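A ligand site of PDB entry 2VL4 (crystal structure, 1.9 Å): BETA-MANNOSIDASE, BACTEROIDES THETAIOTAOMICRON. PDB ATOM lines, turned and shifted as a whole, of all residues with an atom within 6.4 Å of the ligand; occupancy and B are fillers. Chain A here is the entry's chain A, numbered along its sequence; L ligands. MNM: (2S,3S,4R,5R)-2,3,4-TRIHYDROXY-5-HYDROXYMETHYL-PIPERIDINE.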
ATOM      1  N   ASN A 153      13.382  19.357 -27.458  1.00  0.00           N
ATOM      2  CA  ASN A 153      14.580  18.749 -28.079  1.00  0.00           C
ATOM      3  C   ASN A 153      14.551  18.611 -29.606  1.00  0.00           C
ATOM      4  O   ASN A 153      15.575  18.327 -30.196  1.00  0.00           O
ATOM      5  CB  ASN A 153      14.954  17.397 -27.403  1.00  0.00           C
ATOM      6  CG  ASN A 153      15.466  17.589 -25.979  1.00  0.00           C
ATOM      7  OD1 ASN A 153      16.536  18.126 -25.791  1.00  0.00           O
ATOM      8  ND2 ASN A 153      14.683  17.186 -24.983  1.00  0.00           N
ATOM      9  N   TRP A 173      18.861  16.699 -29.996  1.00  0.00           N
ATOM     10  CA  TRP A 173      18.656  16.501 -28.593  1.00  0.00           C
ATOM     11  C   TRP A 173      19.623  17.435 -27.815  1.00  0.00           C
ATOM     12  O   TRP A 173      20.460  18.145 -28.439  1.00  0.00           O
ATOM     13  CB  TRP A 173      18.837  15.014 -28.177  1.00  0.00           C
ATOM     14  CG  TRP A 173      17.888  14.662 -27.010  1.00  0.00           C
ATOM     15  CD1 TRP A 173      18.214  14.612 -25.688  1.00  0.00           C
ATOM     16  CD2 TRP A 173      16.504  14.300 -27.093  1.00  0.00           C
ATOM     17  NE1 TRP A 173      17.119  14.245 -24.940  1.00  0.00           N
ATOM     18  CE2 TRP A 173      16.047  14.072 -25.774  1.00  0.00           C
ATOM     19  CE3 TRP A 173      15.584  14.152 -28.173  1.00  0.00           C
ATOM     20  CZ2 TRP A 173      14.701  13.737 -25.479  1.00  0.00           C
ATOM     21  CZ3 TRP A 173      14.257  13.778 -27.882  1.00  0.00           C
ATOM     22  CH2 TRP A 173      13.828  13.581 -26.538  1.00  0.00           C
ATOM     23  N   ASP A 174      19.584  17.414 -26.484  1.00  0.00           N
ATOM     24  CA  ASP A 174      20.489  18.320 -25.708  1.00  0.00           C
ATOM     25  C   ASP A 174      21.969  17.814 -25.603  1.00  0.00           C
ATOM     26  O   ASP A 174      22.798  18.454 -24.932  1.00  0.00           O
ATOM     27  CB  ASP A 174      19.902  18.721 -24.347  1.00  0.00           C
ATOM     28  CG  ASP A 174      19.617  17.514 -23.429  1.00  0.00           C
ATOM     29  OD1 ASP A 174      20.090  16.359 -23.653  1.00  0.00           O
ATOM     30  OD2 ASP A 174      18.907  17.724 -22.456  1.00  0.00           O
ATOM     31  N   TRP A 175      22.290  16.714 -26.315  1.00  0.00           N
ATOM     32  CA  TRP A 175      23.672  16.257 -26.565  1.00  0.00           C
ATOM     33  C   TRP A 175      23.855  15.868 -28.026  1.00  0.00           C
ATOM     34  O   TRP A 175      24.834  15.209 -28.391  1.00  0.00           O
ATOM     35  CB  TRP A 175      24.011  15.044 -25.675  1.00  0.00           C
ATOM     36  CG  TRP A 175      22.824  14.136 -25.475  1.00  0.00           C
ATOM     37  CD1 TRP A 175      22.080  14.019 -24.353  1.00  0.00           C
ATOM     38  CD2 TRP A 175      22.244  13.237 -26.450  1.00  0.00           C
ATOM     39  NE1 TRP A 175      21.048  13.086 -24.533  1.00  0.00           N
ATOM     40  CE2 TRP A 175      21.138  12.602 -25.818  1.00  0.00           C
ATOM     41  CE3 TRP A 175      22.553  12.922 -27.799  1.00  0.00           C
ATOM     42  CZ2 TRP A 175      20.340  11.661 -26.475  1.00  0.00           C
ATOM     43  CZ3 TRP A 175      21.717  11.977 -28.481  1.00  0.00           C
ATOM     44  CH2 TRP A 175      20.629  11.366 -27.788  1.00  0.00           C
ATOM     45  N   ASN A 336      22.653   4.872 -18.564  1.00  0.00           N
ATOM     46  CA  ASN A 336      21.716   5.098 -19.688  1.00  0.00           C
ATOM     47  C   ASN A 336      22.409   5.093 -21.055  1.00  0.00           C
ATOM     48  O   ASN A 336      23.434   5.771 -21.269  1.00  0.00           O
ATOM     49  CB  ASN A 336      20.957   6.437 -19.464  1.00  0.00           C
ATOM     50  CG  ASN A 336      19.957   6.331 -18.299  1.00  0.00           C
ATOM     51  OD1 ASN A 336      18.767   6.068 -18.491  1.00  0.00           O
ATOM     52  ND2 ASN A 336      20.437   6.611 -17.074  1.00  0.00           N
ATOM     53  N   ARG A 368      20.105   0.961 -19.367  1.00  0.00           N
ATOM     54  CA  ARG A 368      18.791   1.458 -19.755  1.00  0.00           C
ATOM     55  C   ARG A 368      18.840   1.950 -21.195  1.00  0.00           C
ATOM     56  O   ARG A 368      19.634   2.868 -21.520  1.00  0.00           O
ATOM     57  CB  ARG A 368      18.310   2.570 -18.820  1.00  0.00           C
ATOM     58  CG  ARG A 368      17.053   3.323 -19.427  1.00  0.00           C
ATOM     59  CD  ARG A 368      16.278   4.046 -18.313  1.00  0.00           C
ATOM     60  NE  ARG A 368      15.209   4.863 -18.897  1.00  0.00           N
ATOM     61  CZ  ARG A 368      15.108   6.189 -18.778  1.00  0.00           C
ATOM     62  NH1 ARG A 368      16.060   6.865 -18.127  1.00  0.00           N
ATOM     63  NH2 ARG A 368      14.056   6.865 -19.337  1.00  0.00           N
ATOM     64  N   TRP A 370      17.315   4.045 -23.375  1.00  0.00           N
ATOM     65  CA  TRP A 370      16.501   5.251 -23.219  1.00  0.00           C
ATOM     66  C   TRP A 370      15.595   5.549 -24.413  1.00  0.00           C
ATOM     67  O   TRP A 370      15.976   5.392 -25.580  1.00  0.00           O
ATOM     68  CB  TRP A 370      17.468   6.404 -22.961  1.00  0.00           C
ATOM     69  CG  TRP A 370      16.953   7.785 -23.083  1.00  0.00           C
ATOM     70  CD1 TRP A 370      16.340   8.522 -22.091  1.00  0.00           C
ATOM     71  CD2 TRP A 370      17.095   8.651 -24.216  1.00  0.00           C
ATOM     72  NE1 TRP A 370      16.059   9.805 -22.575  1.00  0.00           N
ATOM     73  CE2 TRP A 370      16.515   9.915 -23.861  1.00  0.00           C
ATOM     74  CE3 TRP A 370      17.641   8.491 -25.504  1.00  0.00           C
ATOM     75  CZ2 TRP A 370      16.465  10.988 -24.739  1.00  0.00           C
ATOM     76  CZ3 TRP A 370      17.591   9.565 -26.382  1.00  0.00           C
ATOM     77  CH2 TRP A 370      17.006  10.797 -25.996  1.00  0.00           C
ATOM     78  N   ALA A 398       9.713  10.198 -25.614  1.00  0.00           N
ATOM     79  CA  ALA A 398      10.568  10.876 -24.603  1.00  0.00           C
ATOM     80  C   ALA A 398      10.283  12.358 -24.499  1.00  0.00           C
ATOM     81  O   ALA A 398      10.336  13.035 -25.534  1.00  0.00           O
ATOM     82  CB  ALA A 398      12.066  10.673 -24.945  1.00  0.00           C
ATOM     83  N   CYS A 399      10.030  12.818 -23.276  1.00  0.00           N
ATOM     84  CA  CYS A 399      10.029  14.249 -22.882  1.00  0.00           C
ATOM     85  C   CYS A 399       8.926  15.144 -23.417  1.00  0.00           C
ATOM     86  O   CYS A 399       8.936  16.346 -23.148  1.00  0.00           O
ATOM     87  CB  CYS A 399      11.358  14.919 -23.210  1.00  0.00           C
ATOM     88  SG  CYS A 399      12.814  14.188 -22.440  1.00  0.00           S
ATOM     89  N   ASN A 436      10.206   8.060 -21.298  1.00  0.00           N
ATOM     90  CA  ASN A 436      11.086   8.905 -20.505  1.00  0.00           C
ATOM     91  C   ASN A 436      10.474  10.276 -20.227  1.00  0.00           C
ATOM     92  O   ASN A 436      10.240  11.065 -21.179  1.00  0.00           O
ATOM     93  CB  ASN A 436      12.373   9.156 -21.292  1.00  0.00           C
ATOM     94  CG  ASN A 436      13.329  10.029 -20.553  1.00  0.00           C
ATOM     95  OD1 ASN A 436      13.913   9.561 -19.588  1.00  0.00           O
ATOM     96  ND2 ASN A 436      13.530  11.284 -21.016  1.00  0.00           N
ATOM     97  N   GLU A 437      10.196  10.515 -18.943  1.00  0.00           N
ATOM     98  CA  GLU A 437       9.917  11.870 -18.394  1.00  0.00           C
ATOM     99  C   GLU A 437       8.659  12.540 -18.880  1.00  0.00           C
ATOM    100  O   GLU A 437       8.474  13.738 -18.610  1.00  0.00           O
ATOM    101  CB  GLU A 437      11.102  12.800 -18.643  1.00  0.00           C
ATOM    102  CG  GLU A 437      12.261  12.484 -17.694  1.00  0.00           C
ATOM    103  CD  GLU A 437      13.577  13.263 -17.989  1.00  0.00           C
ATOM    104  OE1 GLU A 437      13.674  13.990 -19.016  1.00  0.00           O
ATOM    105  OE2 GLU A 437      14.520  13.108 -17.186  1.00  0.00           O
ATOM    106  N   HIS A 506      14.913  10.621 -11.332  1.00  0.00           N
ATOM    107  CA  HIS A 506      15.932  11.271 -12.119  1.00  0.00           C
ATOM    108  C   HIS A 506      16.386  12.473 -11.315  1.00  0.00           C
ATOM    109  O   HIS A 506      15.831  13.544 -11.484  1.00  0.00           O
ATOM    110  CB  HIS A 506      15.297  11.761 -13.440  1.00  0.00           C
ATOM    111  CG  HIS A 506      14.885  10.641 -14.378  1.00  0.00           C
ATOM    112  ND1 HIS A 506      14.564  10.859 -15.696  1.00  0.00           N
ATOM    113  CD2 HIS A 506      14.719   9.314 -14.164  1.00  0.00           C
ATOM    114  CE1 HIS A 506      14.205   9.715 -16.261  1.00  0.00           C
ATOM    115  NE2 HIS A 506      14.326   8.756 -15.369  1.00  0.00           N
ATOM    116  N   TRP A 508      18.027  15.470 -10.987  1.00  0.00           N
ATOM    117  CA  TRP A 508      18.780  16.458 -11.715  1.00  0.00           C
ATOM    118  C   TRP A 508      18.979  17.705 -10.833  1.00  0.00           C
ATOM    119  O   TRP A 508      19.183  18.807 -11.330  1.00  0.00           O
ATOM    120  CB  TRP A 508      18.082  16.789 -13.036  1.00  0.00           C
ATOM    121  CG  TRP A 508      18.350  15.664 -14.017  1.00  0.00           C
ATOM    122  CD1 TRP A 508      17.497  14.675 -14.377  1.00  0.00           C
ATOM    123  CD2 TRP A 508      19.588  15.396 -14.662  1.00  0.00           C
ATOM    124  NE1 TRP A 508      18.107  13.811 -15.259  1.00  0.00           N
ATOM    125  CE2 TRP A 508      19.408  14.222 -15.433  1.00  0.00           C
ATOM    126  CE3 TRP A 508      20.856  16.040 -14.659  1.00  0.00           C
ATOM    127  CZ2 TRP A 508      20.429  13.676 -16.229  1.00  0.00           C
ATOM    128  CZ3 TRP A 508      21.879  15.505 -15.424  1.00  0.00           C
ATOM    129  CH2 TRP A 508      21.652  14.324 -16.230  1.00  0.00           C
ATOM    130  N   TRP A 511      23.662  19.332 -11.437  1.00  0.00           N
ATOM    131  CA  TRP A 511      23.551  19.884 -12.812  1.00  0.00           C
ATOM    132  C   TRP A 511      22.399  20.914 -12.906  1.00  0.00           C
ATOM    133  O   TRP A 511      22.628  22.073 -12.608  1.00  0.00           O
ATOM    134  CB  TRP A 511      23.529  18.789 -13.937  1.00  0.00           C
ATOM    135  CG  TRP A 511      23.679  19.438 -15.306  1.00  0.00           C
ATOM    136  CD1 TRP A 511      22.672  19.713 -16.185  1.00  0.00           C
ATOM    137  CD2 TRP A 511      24.880  19.952 -15.903  1.00  0.00           C
ATOM    138  NE1 TRP A 511      23.175  20.347 -17.298  1.00  0.00           N
ATOM    139  CE2 TRP A 511      24.527  20.507 -17.144  1.00  0.00           C
ATOM    140  CE3 TRP A 511      26.238  20.004 -15.490  1.00  0.00           C
ATOM    141  CZ2 TRP A 511      25.480  21.108 -17.995  1.00  0.00           C
ATOM    142  CZ3 TRP A 511      27.174  20.626 -16.335  1.00  0.00           C
ATOM    143  CH2 TRP A 511      26.796  21.153 -17.577  1.00  0.00           C
ATOM    144  N   TYR A 512      21.178  20.506 -13.278  1.00  0.00           N
ATOM    145  CA  TYR A 512      20.055  21.464 -13.456  1.00  0.00           C
ATOM    146  C   TYR A 512      19.700  22.281 -12.218  1.00  0.00           C
ATOM    147  O   TYR A 512      19.447  23.470 -12.373  1.00  0.00           O
ATOM    148  CB  TYR A 512      18.792  20.830 -14.068  1.00  0.00           C
ATOM    149  CG  TYR A 512      19.030  20.391 -15.494  1.00  0.00           C
ATOM    150  CD1 TYR A 512      19.290  21.330 -16.473  1.00  0.00           C
ATOM    151  CD2 TYR A 512      19.094  19.013 -15.841  1.00  0.00           C
ATOM    152  CE1 TYR A 512      19.560  20.952 -17.804  1.00  0.00           C
ATOM    153  CE2 TYR A 512      19.351  18.612 -17.191  1.00  0.00           C
ATOM    154  CZ  TYR A 512      19.596  19.609 -18.158  1.00  0.00           C
ATOM    155  OH  TYR A 512      19.874  19.328 -19.485  1.00  0.00           O
ATOM    156  N   GLU A 530      18.306   8.096 -13.299  1.00  0.00           N
ATOM    157  CA  GLU A 530      19.165   9.096 -13.982  1.00  0.00           C
ATOM    158  C   GLU A 530      19.777  10.054 -12.967  1.00  0.00           C
ATOM    159  O   GLU A 530      19.099  10.479 -12.050  1.00  0.00           O
ATOM    160  CB  GLU A 530      18.390   9.996 -14.977  1.00  0.00           C
ATOM    161  CG  GLU A 530      17.926   9.313 -16.258  1.00  0.00           C
ATOM    162  CD  GLU A 530      17.364  10.303 -17.283  1.00  0.00           C
ATOM    163  OE1 GLU A 530      17.524  11.537 -17.044  1.00  0.00           O
ATOM    164  OE2 GLU A 530      16.825   9.857 -18.321  1.00  0.00           O
ATOM    165  N   TRP A 620      23.422   9.100 -16.026  1.00  0.00           N
ATOM    166  CA  TRP A 620      23.194   9.699 -17.309  1.00  0.00           C
ATOM    167  C   TRP A 620      24.571  10.326 -17.706  1.00  0.00           C
ATOM    168  O   TRP A 620      24.958  11.315 -17.100  1.00  0.00           O
ATOM    169  CB  TRP A 620      22.088  10.794 -17.257  1.00  0.00           C
ATOM    170  CG  TRP A 620      21.862  11.249 -18.636  1.00  0.00           C
ATOM    171  CD1 TRP A 620      22.554  12.223 -19.351  1.00  0.00           C
ATOM    172  CD2 TRP A 620      20.996  10.608 -19.586  1.00  0.00           C
ATOM    173  NE1 TRP A 620      22.118  12.236 -20.680  1.00  0.00           N
ATOM    174  CE2 TRP A 620      21.161  11.261 -20.832  1.00  0.00           C
ATOM    175  CE3 TRP A 620      20.087   9.531 -19.484  1.00  0.00           C
ATOM    176  CZ2 TRP A 620      20.448  10.863 -21.988  1.00  0.00           C
ATOM    177  CZ3 TRP A 620      19.357   9.155 -20.633  1.00  0.00           C
ATOM    178  CH2 TRP A 620      19.539   9.820 -21.850  1.00  0.00           C
ATOM    179  N   GLN A 621      25.294   9.838 -18.729  1.00  0.00           N
ATOM    180  CA  GLN A 621      24.912   8.884 -19.745  1.00  0.00           C
ATOM    181  C   GLN A 621      26.183   8.082 -20.079  1.00  0.00           C
ATOM    182  O   GLN A 621      27.322   8.545 -19.833  1.00  0.00           O
ATOM    183  CB  GLN A 621      24.379   9.597 -21.030  1.00  0.00           C
ATOM    184  CG  GLN A 621      25.473  10.329 -21.868  1.00  0.00           C
ATOM    185  CD  GLN A 621      24.906  11.457 -22.720  1.00  0.00           C
ATOM    186  OE1 GLN A 621      24.498  12.483 -22.203  1.00  0.00           O
ATOM    187  NE2 GLN A 621      24.890  11.276 -24.037  1.00  0.00           N
ATOM    188  N   TRP A 631      27.148  14.617 -20.981  1.00  0.00           N
ATOM    189  CA  TRP A 631      27.208  13.840 -19.751  1.00  0.00           C
ATOM    190  C   TRP A 631      27.891  12.468 -19.874  1.00  0.00           C
ATOM    191  O   TRP A 631      27.914  11.731 -18.933  1.00  0.00           O
ATOM    192  CB  TRP A 631      25.790  13.664 -19.221  1.00  0.00           C
ATOM    193  CG  TRP A 631      25.034  14.997 -19.034  1.00  0.00           C
ATOM    194  CD1 TRP A 631      24.872  15.671 -17.864  1.00  0.00           C
ATOM    195  CD2 TRP A 631      24.342  15.762 -20.037  1.00  0.00           C
ATOM    196  NE1 TRP A 631      24.117  16.832 -18.081  1.00  0.00           N
ATOM    197  CE2 TRP A 631      23.794  16.912 -19.404  1.00  0.00           C
ATOM    198  CE3 TRP A 631      24.127  15.596 -21.426  1.00  0.00           C
ATOM    199  CZ2 TRP A 631      23.033  17.889 -20.098  1.00  0.00           C
ATOM    200  CZ3 TRP A 631      23.357  16.590 -22.109  1.00  0.00           C
ATOM    201  CH2 TRP A 631      22.854  17.718 -21.440  1.00  0.00           C
HETATM  202  C1  MNM L   1      17.546  12.987 -21.508  1.00  0.00           C
HETATM  203  C2  MNM L   1      17.310  12.343 -20.131  1.00  0.00           C
HETATM  204  C3  MNM L   1      18.460  14.223 -21.388  1.00  0.00           C
HETATM  205  O4  MNM L   1      16.301  13.371 -22.105  1.00  0.00           O
HETATM  206  O5  MNM L   1      16.134  11.536 -20.059  1.00  0.00           O
HETATM  207  N6  MNM L   1      17.153  13.327 -19.068  1.00  0.00           N
HETATM  208  O7  MNM L   1      19.373  14.275 -22.501  1.00  0.00           O
HETATM  209  C8  MNM L   1      19.214  14.327 -20.029  1.00  0.00           C
HETATM  210  C9  MNM L   1      20.202  15.514 -19.957  1.00  0.00           C
HETATM  211  C10 MNM L   1      18.154  14.392 -18.919  1.00  0.00           C
HETATM  212  O11 MNM L   1      19.512  16.748 -20.036  1.00  0.00           O
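CZ2 of Trp 508 touches C10 of the ligand, at 3.6 Å. CZ2 of Trp 620 touches O7 of the ligand, 3.6 Å away. Trp 631 touches the ligand (CZ2 to C9, 3.7 Å). The nearest printed residue that does not touch the ligand is His 506 (4.6 Å).
OE1 of Glu 530 is in hydrogen-bond range of NE1 of Trp 508, at 2.9 Å. The guanidinium group (NH1) of Arg 368 is in salt-bridge range of the side-chain carboxylate (OE2) of Glu 530, 3.1 Å away. OE1 of Gln 621 lies within hydrogen-bond range of NE1 of Trp 620 (2.8 Å). The backbone NH (N) of Cys 399 lies within hydrogen-bond range of the backbone carbonyl oxygen (O) of Asn 436 (2.7 Å). The backbone carbonyl oxygen of Trp 631 sits at hydrogen-bond distance from the backbone NH of Gln 621, 3.2 Å away. A ring nitrogen (ND1) of His 506 lies close to the side-chain carboxylate (OE1) of Glu 530 (3.3 Å). The side-chain carboxylate of Glu 530 sits close to the side-chain amide oxygen of Asn 436 (3.2 Å). The side-chain amide oxygen (OD1) of Asn 436 is in hydrogen-bond range of the guanidinium group (NH2) of Arg 368, at 2.7 Å.
OH of Tyr 512 lies within hydrogen-bond range of O11 of the ligand. The side-chain amide nitrogen (ND2) of Asn 436 is in hydrogen-bond range of an oxygen (O5) of the ligand (2.8 Å). An oxygen (O7) of the ligand is in hydrogen-bond range of the side-chain carboxylate of Asp 174, 2.5 Å away. An oxygen (O7) of the ligand is in hydrogen-bond range of the indole nitrogen of Trp 175, 2.9 Å away. NE1 of Trp 173 sits at hydrogen-bond distance from O4 of the ligand, at 3.1 Å. The side-chain sulfur (SG) of Cys 399 lies within hydrogen-bond range of an oxygen (O4) of the ligand, at 3.6 Å. OE1 of Glu 530 lies within salt-bridge range of N6 of the ligand, 2.7 Å away. An oxygen (O5) of the ligand lies within hydrogen-bond range of the indole nitrogen of Trp 370 (3.1 Å). The side-chain carboxylate of Glu 437 is in salt-bridge range of a nitrogen (N6) of the ligand (3.2 Å).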
